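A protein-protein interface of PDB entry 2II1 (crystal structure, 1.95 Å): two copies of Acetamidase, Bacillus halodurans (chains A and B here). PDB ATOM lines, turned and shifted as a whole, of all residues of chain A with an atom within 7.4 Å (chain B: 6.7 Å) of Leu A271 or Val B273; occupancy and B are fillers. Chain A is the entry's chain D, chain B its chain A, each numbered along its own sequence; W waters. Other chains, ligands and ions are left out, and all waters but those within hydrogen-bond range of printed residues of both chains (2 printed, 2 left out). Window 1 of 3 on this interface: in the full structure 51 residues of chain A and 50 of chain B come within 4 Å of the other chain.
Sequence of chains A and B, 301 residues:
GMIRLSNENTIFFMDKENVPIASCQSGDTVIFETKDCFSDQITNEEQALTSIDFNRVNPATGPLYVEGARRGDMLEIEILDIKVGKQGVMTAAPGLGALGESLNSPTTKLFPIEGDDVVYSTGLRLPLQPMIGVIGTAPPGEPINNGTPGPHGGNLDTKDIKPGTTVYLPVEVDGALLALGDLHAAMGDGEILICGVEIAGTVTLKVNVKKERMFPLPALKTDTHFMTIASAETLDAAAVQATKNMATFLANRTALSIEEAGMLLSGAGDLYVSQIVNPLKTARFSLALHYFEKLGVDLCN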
ATOM      1  N   ASP A 189      29.210  22.474 -11.269  1.00  0.00           N
ATOM      2  CA  ASP A 189      28.812  22.725 -12.660  1.00  0.00           C
ATOM      3  C   ASP A 189      28.232  24.164 -12.793  1.00  0.00           C
ATOM      4  O   ASP A 189      27.348  24.582 -12.037  1.00  0.00           O
ATOM      5  CB  ASP A 189      27.775  21.695 -13.186  1.00  0.00           C
ATOM      6  CG  ASP A 189      28.413  20.380 -13.714  1.00  0.00           C
ATOM      7  OD1 ASP A 189      29.647  20.332 -13.965  1.00  0.00           O
ATOM      8  OD2 ASP A 189      27.666  19.380 -13.857  1.00  0.00           O
ATOM      9  N   THR A 228      31.817  14.274 -24.694  1.00  0.00           N
ATOM     10  CA  THR A 228      32.233  15.289 -25.648  1.00  0.00           C
ATOM     11  C   THR A 228      32.004  16.701 -25.120  1.00  0.00           C
ATOM     12  O   THR A 228      30.949  17.002 -24.590  1.00  0.00           O
ATOM     13  CB  THR A 228      31.501  15.093 -26.977  1.00  0.00           C
ATOM     14  OG1 THR A 228      30.098  15.120 -26.746  1.00  0.00           O
ATOM     15  CG2 THR A 228      31.905  13.735 -27.651  1.00  0.00           C
ATOM     16  N   LEU A 235      25.668  29.436 -24.183  1.00  0.00           N
ATOM     17  CA  LEU A 235      25.433  28.085 -23.690  1.00  0.00           C
ATOM     18  C   LEU A 235      24.520  27.314 -24.653  1.00  0.00           C
ATOM     19  O   LEU A 235      24.690  26.111 -24.862  1.00  0.00           O
ATOM     20  CB  LEU A 235      24.852  28.118 -22.268  1.00  0.00           C
ATOM     21  CG  LEU A 235      24.785  26.788 -21.525  1.00  0.00           C
ATOM     22  CD1 LEU A 235      26.182  26.127 -21.344  1.00  0.00           C
ATOM     23  CD2 LEU A 235      24.051  27.028 -20.188  1.00  0.00           C
ATOM     24  N   ASP A 236      23.578  28.018 -25.264  1.00  0.00           N
ATOM     25  CA  ASP A 236      22.699  27.404 -26.249  1.00  0.00           C
ATOM     26  C   ASP A 236      23.484  26.725 -27.374  1.00  0.00           C
ATOM     27  O   ASP A 236      23.175  25.595 -27.765  1.00  0.00           O
ATOM     28  CB  ASP A 236      21.781  28.455 -26.840  1.00  0.00           C
ATOM     29  CG  ASP A 236      20.959  29.175 -25.775  1.00  0.00           C
ATOM     30  OD1 ASP A 236      21.561  29.829 -24.877  1.00  0.00           O
ATOM     31  OD2 ASP A 236      19.718  29.080 -25.835  1.00  0.00           O
ATOM     32  N   ALA A 238      26.886  26.016 -27.300  1.00  0.00           N
ATOM     33  CA  ALA A 238      27.868  25.008 -26.810  1.00  0.00           C
ATOM     34  C   ALA A 238      27.191  23.657 -26.540  1.00  0.00           C
ATOM     35  O   ALA A 238      27.739  22.576 -26.835  1.00  0.00           O
ATOM     36  CB  ALA A 238      28.586  25.501 -25.540  1.00  0.00           C
ATOM     37  N   ALA A 239      25.990  23.730 -25.965  1.00  0.00           N
ATOM     38  CA  ALA A 239      25.142  22.559 -25.719  1.00  0.00           C
ATOM     39  C   ALA A 239      24.799  21.801 -27.010  1.00  0.00           C
ATOM     40  O   ALA A 239      24.907  20.577 -27.063  1.00  0.00           O
ATOM     41  CB  ALA A 239      23.825  22.979 -24.980  1.00  0.00           C
ATOM     42  N   VAL A 240      24.363  22.527 -28.034  1.00  0.00           N
ATOM     43  CA  VAL A 240      24.045  21.910 -29.322  1.00  0.00           C
ATOM     44  C   VAL A 240      25.278  21.265 -29.921  1.00  0.00           C
ATOM     45  O   VAL A 240      25.241  20.087 -30.334  1.00  0.00           O
ATOM     46  CB  VAL A 240      23.405  22.892 -30.302  1.00  0.00           C
ATOM     47  CG1 VAL A 240      23.425  22.318 -31.751  1.00  0.00           C
ATOM     48  CG2 VAL A 240      21.954  23.255 -29.858  1.00  0.00           C
ATOM     49  N   GLN A 241      26.386  22.004 -29.947  1.00  0.00           N
ATOM     50  CA  GLN A 241      27.602  21.467 -30.535  1.00  0.00           C
ATOM     51  C   GLN A 241      28.100  20.244 -29.797  1.00  0.00           C
ATOM     52  O   GLN A 241      28.524  19.290 -30.425  1.00  0.00           O
ATOM     53  CB  GLN A 241      28.740  22.454 -30.563  1.00  0.00           C
ATOM     54  CG  GLN A 241      29.899  21.978 -31.472  1.00  0.00           C
ATOM     55  CD  GLN A 241      29.427  21.688 -32.903  1.00  0.00           C
ATOM     56  OE1 GLN A 241      28.752  22.498 -33.493  1.00  0.00           O
ATOM     57  NE2 GLN A 241      29.746  20.521 -33.419  1.00  0.00           N
ATOM     58  N   ALA A 242      28.121  20.309 -28.479  1.00  0.00           N
ATOM     59  CA  ALA A 242      28.534  19.143 -27.674  1.00  0.00           C
ATOM     60  C   ALA A 242      27.706  17.891 -27.963  1.00  0.00           C
ATOM     61  O   ALA A 242      28.220  16.765 -27.965  1.00  0.00           O
ATOM     62  CB  ALA A 242      28.454  19.469 -26.202  1.00  0.00           C
ATOM     63  N   THR A 243      26.413  18.102 -28.173  1.00  0.00           N
ATOM     64  CA  THR A 243      25.451  17.033 -28.432  1.00  0.00           C
ATOM     65  C   THR A 243      25.686  16.449 -29.808  1.00  0.00           C
ATOM     66  O   THR A 243      25.781  15.220 -29.947  1.00  0.00           O
ATOM     67  CB  THR A 243      23.986  17.559 -28.303  1.00  0.00           C
ATOM     68  OG1 THR A 243      23.802  18.103 -26.978  1.00  0.00           O
ATOM     69  CG2 THR A 243      22.971  16.433 -28.568  1.00  0.00           C
ATOM     70  N   LEU A 265      20.807   8.940 -27.238  1.00  0.00           N
ATOM     71  CA  LEU A 265      21.304  10.053 -26.448  1.00  0.00           C
ATOM     72  C   LEU A 265      20.162  10.718 -25.677  1.00  0.00           C
ATOM     73  O   LEU A 265      20.326  11.074 -24.496  1.00  0.00           O
ATOM     74  CB  LEU A 265      21.987  11.118 -27.318  1.00  0.00           C
ATOM     75  CG  LEU A 265      23.310  10.838 -28.057  1.00  0.00           C
ATOM     76  CD1 LEU A 265      23.998  12.135 -28.556  1.00  0.00           C
ATOM     77  CD2 LEU A 265      24.268  10.055 -27.227  1.00  0.00           C
ATOM     78  N   GLY A 269      21.461   9.433 -22.524  1.00  0.00           N
ATOM     79  CA  GLY A 269      22.554  10.396 -22.321  1.00  0.00           C
ATOM     80  C   GLY A 269      22.160  11.654 -21.554  1.00  0.00           C
ATOM     81  O   GLY A 269      20.982  11.940 -21.379  1.00  0.00           O
ATOM     82  N   ASP A 270      23.155  12.418 -21.114  1.00  0.00           N
ATOM     83  CA  ASP A 270      22.946  13.645 -20.367  1.00  0.00           C
ATOM     84  C   ASP A 270      23.804  14.807 -20.863  1.00  0.00           C
ATOM     85  O   ASP A 270      25.033  14.717 -21.005  1.00  0.00           O
ATOM     86  CB  ASP A 270      23.230  13.426 -18.889  1.00  0.00           C
ATOM     87  CG  ASP A 270      22.239  12.467 -18.229  1.00  0.00           C
ATOM     88  OD1 ASP A 270      21.061  12.854 -18.003  1.00  0.00           O
ATOM     89  OD2 ASP A 270      22.652  11.335 -17.908  1.00  0.00           O
ATOM     90  N   LEU A 271      23.135  15.916 -21.124  1.00  0.00           N
ATOM     91  CA  LEU A 271      23.809  17.164 -21.398  1.00  0.00           C
ATOM     92  C   LEU A 271      24.072  17.900 -20.071  1.00  0.00           C
ATOM     93  O   LEU A 271      23.167  18.139 -19.314  1.00  0.00           O
ATOM     94  CB  LEU A 271      22.956  17.998 -22.321  1.00  0.00           C
ATOM     95  CG  LEU A 271      23.507  19.328 -22.834  1.00  0.00           C
ATOM     96  CD1 LEU A 271      24.829  19.150 -23.587  1.00  0.00           C
ATOM     97  CD2 LEU A 271      22.410  19.903 -23.682  1.00  0.00           C
ATOM     98  N   TYR A 272      25.334  18.234 -19.832  1.00  0.00           N
ATOM     99  CA  TYR A 272      25.802  18.961 -18.659  1.00  0.00           C
ATOM    100  C   TYR A 272      26.468  20.304 -19.010  1.00  0.00           C
ATOM    101  O   TYR A 272      26.911  20.533 -20.131  1.00  0.00           O
ATOM    102  CB  TYR A 272      26.800  18.097 -17.857  1.00  0.00           C
ATOM    103  CG  TYR A 272      26.225  16.831 -17.273  1.00  0.00           C
ATOM    104  CD1 TYR A 272      25.144  16.872 -16.383  1.00  0.00           C
ATOM    105  CD2 TYR A 272      26.743  15.583 -17.620  1.00  0.00           C
ATOM    106  CE1 TYR A 272      24.626  15.661 -15.802  1.00  0.00           C
ATOM    107  CE2 TYR A 272      26.221  14.406 -17.078  1.00  0.00           C
ATOM    108  CZ  TYR A 272      25.153  14.451 -16.190  1.00  0.00           C
ATOM    109  OH  TYR A 272      24.673  13.275 -15.651  1.00  0.00           O
ATOM    110  N   VAL A 273      26.507  21.187 -18.012  1.00  0.00           N
ATOM    111  CA  VAL A 273      27.078  22.531 -18.111  1.00  0.00           C
ATOM    112  C   VAL A 273      28.426  22.470 -17.410  1.00  0.00           C
ATOM    113  O   VAL A 273      28.520  21.930 -16.297  1.00  0.00           O
ATOM    114  CB  VAL A 273      26.201  23.572 -17.372  1.00  0.00           C
ATOM    115  CG1 VAL A 273      26.753  24.959 -17.533  1.00  0.00           C
ATOM    116  CG2 VAL A 273      24.758  23.477 -17.861  1.00  0.00           C
ATOM    117  N   ALA A 283      29.929  23.385 -22.364  1.00  0.00           N
ATOM    118  CA  ALA A 283      28.990  22.283 -22.044  1.00  0.00           C
ATOM    119  C   ALA A 283      29.626  20.942 -22.464  1.00  0.00           C
ATOM    120  O   ALA A 283      30.555  20.898 -23.256  1.00  0.00           O
ATOM    121  CB  ALA A 283      27.624  22.490 -22.735  1.00  0.00           C
ATOM    122  N   ARG A 284      29.166  19.852 -21.855  1.00  0.00           N
ATOM    123  CA  ARG A 284      29.600  18.520 -22.224  1.00  0.00           C
ATOM    124  C   ARG A 284      28.377  17.566 -22.334  1.00  0.00           C
ATOM    125  O   ARG A 284      27.413  17.664 -21.550  1.00  0.00           O
ATOM    126  CB  ARG A 284      30.689  18.009 -21.238  1.00  0.00           C
ATOM    127  CG  ARG A 284      30.309  18.017 -19.778  1.00  0.00           C
ATOM    128  CD  ARG A 284      31.500  17.782 -18.877  1.00  0.00           C
ATOM    129  NE  ARG A 284      31.103  17.407 -17.528  1.00  0.00           N
ATOM    130  CZ  ARG A 284      30.643  18.268 -16.623  1.00  0.00           C
ATOM    131  NH1 ARG A 284      30.512  19.520 -16.943  1.00  0.00           N
ATOM    132  NH2 ARG A 284      30.299  17.879 -15.399  1.00  0.00           N
ATOM    133  N   PHE A 285      28.405  16.679 -23.336  1.00  0.00           N
ATOM    134  CA  PHE A 285      27.416  15.624 -23.444  1.00  0.00           C
ATOM    135  C   PHE A 285      28.024  14.306 -23.005  1.00  0.00           C
ATOM    136  O   PHE A 285      29.088  13.948 -23.496  1.00  0.00           O
ATOM    137  CB  PHE A 285      26.862  15.454 -24.869  1.00  0.00           C
ATOM    138  CG  PHE A 285      25.593  14.680 -24.866  1.00  0.00           C
ATOM    139  CD1 PHE A 285      25.608  13.281 -24.789  1.00  0.00           C
ATOM    140  CD2 PHE A 285      24.375  15.334 -24.787  1.00  0.00           C
ATOM    141  CE1 PHE A 285      24.424  12.571 -24.718  1.00  0.00           C
ATOM    142  CE2 PHE A 285      23.192  14.620 -24.724  1.00  0.00           C
ATOM    143  CZ  PHE A 285      23.228  13.239 -24.675  1.00  0.00           C
ATOM    144  N   SER A 286      27.306  13.567 -22.138  1.00  0.00           N
ATOM    145  CA  SER A 286      27.800  12.400 -21.447  1.00  0.00           C
ATOM    146  C   SER A 286      26.943  11.128 -21.638  1.00  0.00           C
ATOM    147  O   SER A 286      25.731  11.165 -21.476  1.00  0.00           O
ATOM    148  CB  SER A 286      27.838  12.770 -19.971  1.00  0.00           C
ATOM    149  OG  SER A 286      28.297  11.711 -19.194  1.00  0.00           O
ATOM    150  N   ASP B 157      10.045  18.937 -18.720  1.00  0.00           N
ATOM    151  CA  ASP B 157      10.896  17.788 -19.023  1.00  0.00           C
ATOM    152  C   ASP B 157      12.132  17.675 -18.122  1.00  0.00           C
ATOM    153  O   ASP B 157      13.277  17.674 -18.584  1.00  0.00           O
ATOM    154  CB  ASP B 157      11.227  17.750 -20.521  1.00  0.00           C
ATOM    155  CG  ASP B 157       9.995  17.506 -21.372  1.00  0.00           C
ATOM    156  OD1 ASP B 157       9.065  16.817 -20.891  1.00  0.00           O
ATOM    157  OD2 ASP B 157       9.945  17.987 -22.517  1.00  0.00           O
ATOM    158  N   THR B 158      11.859  17.545 -16.822  1.00  0.00           N
ATOM    159  CA  THR B 158      12.875  17.479 -15.774  1.00  0.00           C
ATOM    160  C   THR B 158      12.848  16.070 -15.212  1.00  0.00           C
ATOM    161  O   THR B 158      11.831  15.620 -14.653  1.00  0.00           O
ATOM    162  CB  THR B 158      12.598  18.595 -14.700  1.00  0.00           C
ATOM    163  OG1 THR B 158      12.799  19.872 -15.307  1.00  0.00           O
ATOM    164  CG2 THR B 158      13.489  18.498 -13.472  1.00  0.00           C
ATOM    165  N   LYS B 159      13.963  15.359 -15.374  1.00  0.00           N
ATOM    166  CA  LYS B 159      14.037  13.943 -15.041  1.00  0.00           C
ATOM    167  C   LYS B 159      14.035  13.665 -13.542  1.00  0.00           C
ATOM    168  O   LYS B 159      13.808  12.528 -13.111  1.00  0.00           O
ATOM    169  CB  LYS B 159      15.240  13.256 -15.748  1.00  0.00           C
ATOM    170  CG  LYS B 159      16.608  13.432 -15.078  1.00  0.00           C
ATOM    171  CD  LYS B 159      17.698  12.658 -15.804  1.00  0.00           C
ATOM    172  CE  LYS B 159      19.037  12.878 -15.125  1.00  0.00           C
ATOM    173  NZ  LYS B 159      20.169  12.097 -15.705  1.00  0.00           N
ATOM    174  N   MET B 187      14.633   9.139 -20.096  1.00  0.00           N
ATOM    175  CA  MET B 187      14.995  10.432 -20.698  1.00  0.00           C
ATOM    176  C   MET B 187      16.232  10.955 -19.975  1.00  0.00           C
ATOM    177  O   MET B 187      16.336  10.864 -18.757  1.00  0.00           O
ATOM    178  CB  MET B 187      13.882  11.465 -20.530  1.00  0.00           C
ATOM    179  CG  MET B 187      13.984  12.651 -21.489  1.00  0.00           C
ATOM    180  SD  MET B 187      13.122  14.229 -20.746  1.00  0.00           S
ATOM    181  CE  MET B 187      14.488  14.852 -19.477  1.00  0.00           C
ATOM    182  N   GLY B 188      17.153  11.521 -20.741  1.00  0.00           N
ATOM    183  CA  GLY B 188      18.351  12.142 -20.196  1.00  0.00           C
ATOM    184  C   GLY B 188      18.263  13.653 -20.206  1.00  0.00           C
ATOM    185  O   GLY B 188      17.477  14.228 -20.952  1.00  0.00           O
ATOM    186  N   ASP B 189      19.055  14.294 -19.352  1.00  0.00           N
ATOM    187  CA  ASP B 189      19.125  15.748 -19.322  1.00  0.00           C
ATOM    188  C   ASP B 189      19.314  16.285 -20.749  1.00  0.00           C
ATOM    189  O   ASP B 189      20.160  15.805 -21.534  1.00  0.00           O
ATOM    190  CB  ASP B 189      20.254  16.238 -18.409  1.00  0.00           C
ATOM    191  CG  ASP B 189      19.870  16.239 -16.934  1.00  0.00           C
ATOM    192  OD1 ASP B 189      18.655  16.099 -16.594  1.00  0.00           O
ATOM    193  OD2 ASP B 189      20.797  16.391 -16.115  1.00  0.00           O
ATOM    194  N   GLY B 190      18.515  17.281 -21.093  1.00  0.00           N
ATOM    195  CA  GLY B 190      18.574  17.842 -22.429  1.00  0.00           C
ATOM    196  C   GLY B 190      17.474  17.387 -23.367  1.00  0.00           C
ATOM    197  O   GLY B 190      17.065  18.154 -24.239  1.00  0.00           O
ATOM    198  N   GLU B 191      16.970  16.170 -23.196  1.00  0.00           N
ATOM    199  CA  GLU B 191      15.919  15.660 -24.110  1.00  0.00           C
ATOM    200  C   GLU B 191      16.244  16.035 -25.575  1.00  0.00           C
ATOM    201  O   GLU B 191      15.391  16.522 -26.330  1.00  0.00           O
ATOM    202  CB  GLU B 191      14.569  16.231 -23.716  1.00  0.00           C
ATOM    203  CG  GLU B 191      13.411  15.437 -24.284  1.00  0.00           C
ATOM    204  CD  GLU B 191      12.071  16.022 -23.934  1.00  0.00           C
ATOM    205  OE1 GLU B 191      12.000  17.268 -23.800  1.00  0.00           O
ATOM    206  OE2 GLU B 191      11.096  15.230 -23.801  1.00  0.00           O
ATOM    207  N   ILE B 192      17.496  15.794 -25.964  1.00  0.00           N
ATOM    208  CA  ILE B 192      18.071  16.448 -27.144  1.00  0.00           C
ATOM    209  C   ILE B 192      17.425  16.099 -28.492  1.00  0.00           C
ATOM    210  O   ILE B 192      17.427  16.921 -29.377  1.00  0.00           O
ATOM    211  CB  ILE B 192      19.636  16.310 -27.236  1.00  0.00           C
ATOM    212  CG1 ILE B 192      20.095  14.846 -27.432  1.00  0.00           C
ATOM    213  CG2 ILE B 192      20.273  16.984 -26.028  1.00  0.00           C
ATOM    214  CD1 ILE B 192      20.068  14.334 -28.914  1.00  0.00           C
ATOM    215  N   LEU B 235      18.756  28.914 -23.245  1.00  0.00           N
ATOM    216  CA  LEU B 235      19.317  28.157 -22.156  1.00  0.00           C
ATOM    217  C   LEU B 235      20.265  29.042 -21.316  1.00  0.00           C
ATOM    218  O   LEU B 235      20.395  28.826 -20.122  1.00  0.00           O
ATOM    219  CB  LEU B 235      20.025  26.912 -22.675  1.00  0.00           C
ATOM    220  CG  LEU B 235      20.591  25.952 -21.637  1.00  0.00           C
ATOM    221  CD1 LEU B 235      19.493  25.328 -20.716  1.00  0.00           C
ATOM    222  CD2 LEU B 235      21.383  24.864 -22.400  1.00  0.00           C
ATOM    223  N   LEU B 271      24.684  23.432 -11.660  1.00  0.00           N
ATOM    224  CA  LEU B 271      23.706  23.887 -12.606  1.00  0.00           C
ATOM    225  C   LEU B 271      23.502  22.755 -13.585  1.00  0.00           C
ATOM    226  O   LEU B 271      24.445  22.276 -14.176  1.00  0.00           O
ATOM    227  CB  LEU B 271      24.211  25.127 -13.360  1.00  0.00           C
ATOM    228  CG  LEU B 271      23.323  25.738 -14.426  1.00  0.00           C
ATOM    229  CD1 LEU B 271      22.017  26.247 -13.837  1.00  0.00           C
ATOM    230  CD2 LEU B 271      24.144  26.848 -15.105  1.00  0.00           C
ATOM    231  N   TYR B 272      22.247  22.360 -13.762  1.00  0.00           N
ATOM    232  CA  TYR B 272      21.860  21.293 -14.675  1.00  0.00           C
ATOM    233  C   TYR B 272      20.854  21.781 -15.711  1.00  0.00           C
ATOM    234  O   TYR B 272      20.136  22.758 -15.505  1.00  0.00           O
ATOM    235  CB  TYR B 272      21.199  20.142 -13.911  1.00  0.00           C
ATOM    236  CG  TYR B 272      22.085  19.382 -12.941  1.00  0.00           C
ATOM    237  CD1 TYR B 272      23.224  18.693 -13.392  1.00  0.00           C
ATOM    238  CD2 TYR B 272      21.783  19.335 -11.583  1.00  0.00           C
ATOM    239  CE1 TYR B 272      24.031  17.988 -12.519  1.00  0.00           C
ATOM    240  CE2 TYR B 272      22.582  18.617 -10.699  1.00  0.00           C
ATOM    241  CZ  TYR B 272      23.705  17.955 -11.177  1.00  0.00           C
ATOM    242  OH  TYR B 272      24.484  17.248 -10.311  1.00  0.00           O
ATOM    243  N   VAL B 273      20.802  21.024 -16.795  1.00  0.00           N
ATOM    244  CA  VAL B 273      19.941  21.251 -17.935  1.00  0.00           C
ATOM    245  C   VAL B 273      18.795  20.253 -17.873  1.00  0.00           C
ATOM    246  O   VAL B 273      19.025  19.054 -17.690  1.00  0.00           O
ATOM    247  CB  VAL B 273      20.739  21.029 -19.246  1.00  0.00           C
ATOM    248  CG1 VAL B 273      19.820  20.812 -20.425  1.00  0.00           C
ATOM    249  CG2 VAL B 273      21.733  22.183 -19.501  1.00  0.00           C
ATOM    250  N   SER B 274      17.565  20.738 -18.028  1.00  0.00           N
ATOM    251  CA  SER B 274      16.403  19.862 -18.047  1.00  0.00           C
ATOM    252  C   SER B 274      16.116  19.404 -19.463  1.00  0.00           C
ATOM    253  O   SER B 274      16.106  18.211 -19.727  1.00  0.00           O
ATOM    254  CB  SER B 274      15.156  20.534 -17.448  1.00  0.00           C
ATOM    255  OG  SER B 274      15.249  20.596 -16.031  1.00  0.00           O
ATOM    256  N   GLN B 275      15.853  20.365 -20.349  1.00  0.00           N
ATOM    257  CA  GLN B 275      15.530  20.094 -21.745  1.00  0.00           C
ATOM    258  C   GLN B 275      15.959  21.302 -22.542  1.00  0.00           C
ATOM    259  O   GLN B 275      15.889  22.412 -22.006  1.00  0.00           O
ATOM    260  CB  GLN B 275      14.013  19.851 -21.937  1.00  0.00           C
ATOM    261  CG  GLN B 275      13.057  20.967 -21.444  1.00  0.00           C
ATOM    262  CD  GLN B 275      12.912  22.141 -22.434  1.00  0.00           C
ATOM    263  OE1 GLN B 275      13.257  22.019 -23.621  1.00  0.00           O
ATOM    264  NE2 GLN B 275      12.409  23.277 -21.942  1.00  0.00           N
ATOM    265  N   ILE B 276      16.345  21.114 -23.808  1.00  0.00           N
ATOM    266  CA  ILE B 276      16.675  22.239 -24.713  1.00  0.00           C
ATOM    267  C   ILE B 276      15.843  22.295 -25.992  1.00  0.00           C
ATOM    268  O   ILE B 276      16.219  22.976 -26.979  1.00  0.00           O
ATOM    269  CB  ILE B 276      18.193  22.272 -25.062  1.00  0.00           C
ATOM    270  CG1 ILE B 276      18.625  21.031 -25.844  1.00  0.00           C
ATOM    271  CG2 ILE B 276      19.015  22.368 -23.795  1.00  0.00           C
ATOM    272  CD1 ILE B 276      20.013  21.136 -26.448  1.00  0.00           C
ATOM    273  N   THR B 282      14.654  24.804 -20.319  1.00  0.00           N
ATOM    274  CA  THR B 282      14.537  24.700 -18.859  1.00  0.00           C
ATOM    275  C   THR B 282      15.856  24.231 -18.266  1.00  0.00           C
ATOM    276  O   THR B 282      16.482  23.343 -18.804  1.00  0.00           O
ATOM    277  CB  THR B 282      13.443  23.728 -18.463  1.00  0.00           C
ATOM    278  OG1 THR B 282      12.214  24.148 -19.057  1.00  0.00           O
ATOM    279  CG2 THR B 282      13.284  23.660 -16.929  1.00  0.00           C
ATOM    280  N   ALA B 283      16.243  24.844 -17.152  1.00  0.00           N
ATOM    281  CA  ALA B 283      17.480  24.570 -16.416  1.00  0.00           C
ATOM    282  C   ALA B 283      17.130  24.475 -14.952  1.00  0.00           C
ATOM    283  O   ALA B 283      16.063  24.977 -14.530  1.00  0.00           O
ATOM    284  CB  ALA B 283      18.489  25.682 -16.638  1.00  0.00           C
ATOM    285  N   ARG B 284      17.985  23.802 -14.179  1.00  0.00           N
ATOM    286  CA  ARG B 284      17.817  23.753 -12.705  1.00  0.00           C
ATOM    287  C   ARG B 284      19.119  23.879 -11.957  1.00  0.00           C
ATOM    288  O   ARG B 284      20.134  23.324 -12.371  1.00  0.00           O
ATOM    289  CB  ARG B 284      17.051  22.503 -12.204  1.00  0.00           C
ATOM    290  CG  ARG B 284      17.626  21.162 -12.559  1.00  0.00           C
ATOM    291  CD  ARG B 284      16.531  20.093 -12.613  1.00  0.00           C
ATOM    292  NE  ARG B 284      17.121  18.748 -12.666  1.00  0.00           N
ATOM    293  CZ  ARG B 284      17.629  18.182 -13.757  1.00  0.00           C
ATOM    294  NH1 ARG B 284      17.623  18.815 -14.912  1.00  0.00           N
ATOM    295  NH2 ARG B 284      18.170  16.972 -13.699  1.00  0.00           N
HETATM  296  O   HOH W   1      22.277  18.647 -16.920  1.00  0.00           O
HETATM  297  O   HOH W   2      25.556  20.117 -15.402  1.00  0.00           O
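OD1 of Asp A270 lies within salt-bridge range of NZ of Lys B159, at 2.6 Å.
The backbone NH (N) of Asp B189 sits at hydrogen-bond distance from the side-chain carboxylate (OD1) of Asp A270 (2.8 Å).
The backbone NH (N) of Leu A271 sits at hydrogen-bond distance from the backbone carbonyl oxygen (O) of Asp B189 (3.0 Å).
N of Leu B235 is in hydrogen-bond range of OD2 of Asp A236 (2.8 Å).
The backbone NH (N) of Leu B271 sits at hydrogen-bond distance from the backbone carbonyl oxygen (O) of Asp A189, at 2.9 Å.
The side-chain carboxylate (OD1) of Asp B189 lies within salt-bridge range of the guanidinium group (NH2) of Arg B284 (3.1 Å).
The backbone NH (N) of Ile B276 lies within hydrogen-bond range of the backbone carbonyl oxygen (O) of Gly B190 (3.1 Å).
N of Phe A285 sits at hydrogen-bond distance from O of Thr A228 (2.9 Å).
The backbone carbonyl oxygen (O) of Ala A239 sits at hydrogen-bond distance from the side-chain hydroxyl (OG1) of Thr A243 (2.7 Å).
The backbone carbonyl oxygen (O) of Asp A270 sits at hydrogen-bond distance from the backbone NH (N) of Ser A286 (2.8 Å).
The backbone carbonyl oxygen (O) of Arg A284 lies within hydrogen-bond range of the backbone NH (N) of Tyr A272, at 2.8 Å.
Among the printed residues, merely in contact across the chains: Leu A235 with Leu B235, Thr A243 with Ile B192, Gly A269 with Gly B188, Gly A269 with Asp B189, Asp A270 with Gly B188, Leu A271 with Val B273, Leu A271 with Ile B276, Tyr A272 with Asp B189, Tyr A272 with Tyr B272, Val A273 with Leu B271, Val A273 with Val B273 and Phe A285 with Ile B192.
Val B273 touches just these residues of chain A: Leu A271 and Val A273.
Printed residues of chain B within 4 Å of Leu A235: Leu B235.
Of the printed residues of chain A, Ile B276 touches Leu A271 (3.9 Å).
Of the printed residues of chain B, Tyr A272 touches Asp B189 (3.9 Å) and Tyr B272 (3.99 Å).
Of the printed residues of chain A, Ile B192 touches Thr A243 and Phe A285.
Gln B275 touches none of the printed residues of chain A.
Thr B282 touches none of the printed residues of chain A.
Printed residues of chain A that touch a printed residue of chain B: Asp A189, Leu A235, Asp A236, Thr A243, Gly A269, Asp A270, Leu A271, Tyr A272, Val A273 and Phe A285.
Hydrophobic or aromatic side chains of chain A that line the printed part of chain B: Leu A235, Leu A271, Tyr A272, Val A273 and Phe A285.
Among the printed residues, Asp or Glu carboxylates within 4 Å of a Lys or Arg side-chain nitrogen of the other chain: Asp A270 with Lys B159 (2.6 Å).
Leu B235 touches its own counterpart, Leu A235.
Leu A271 touches Val B273, and with the chains exchanged Val A273 touches Leu B271.
Tyr B272 touches its own counterpart, Tyr A272.
Val A273 touches its own counterpart, Val B273.
7 positions are printed for both chains.
Water W1 lies within hydrogen-bond range of the backbone carbonyl oxygen (O) of Leu A271 (2.6 Å), the backbone NH (N) of Val B273 (2.8 Å) and the side-chain carboxylate (OD2) of Asp B189 (2.8 Å).
Water W2 lies within hydrogen-bond range of OD2 of Asp A189 (2.7 Å), O of Leu B271 (2.7 Å) and N of Val A273 (3.0 Å).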
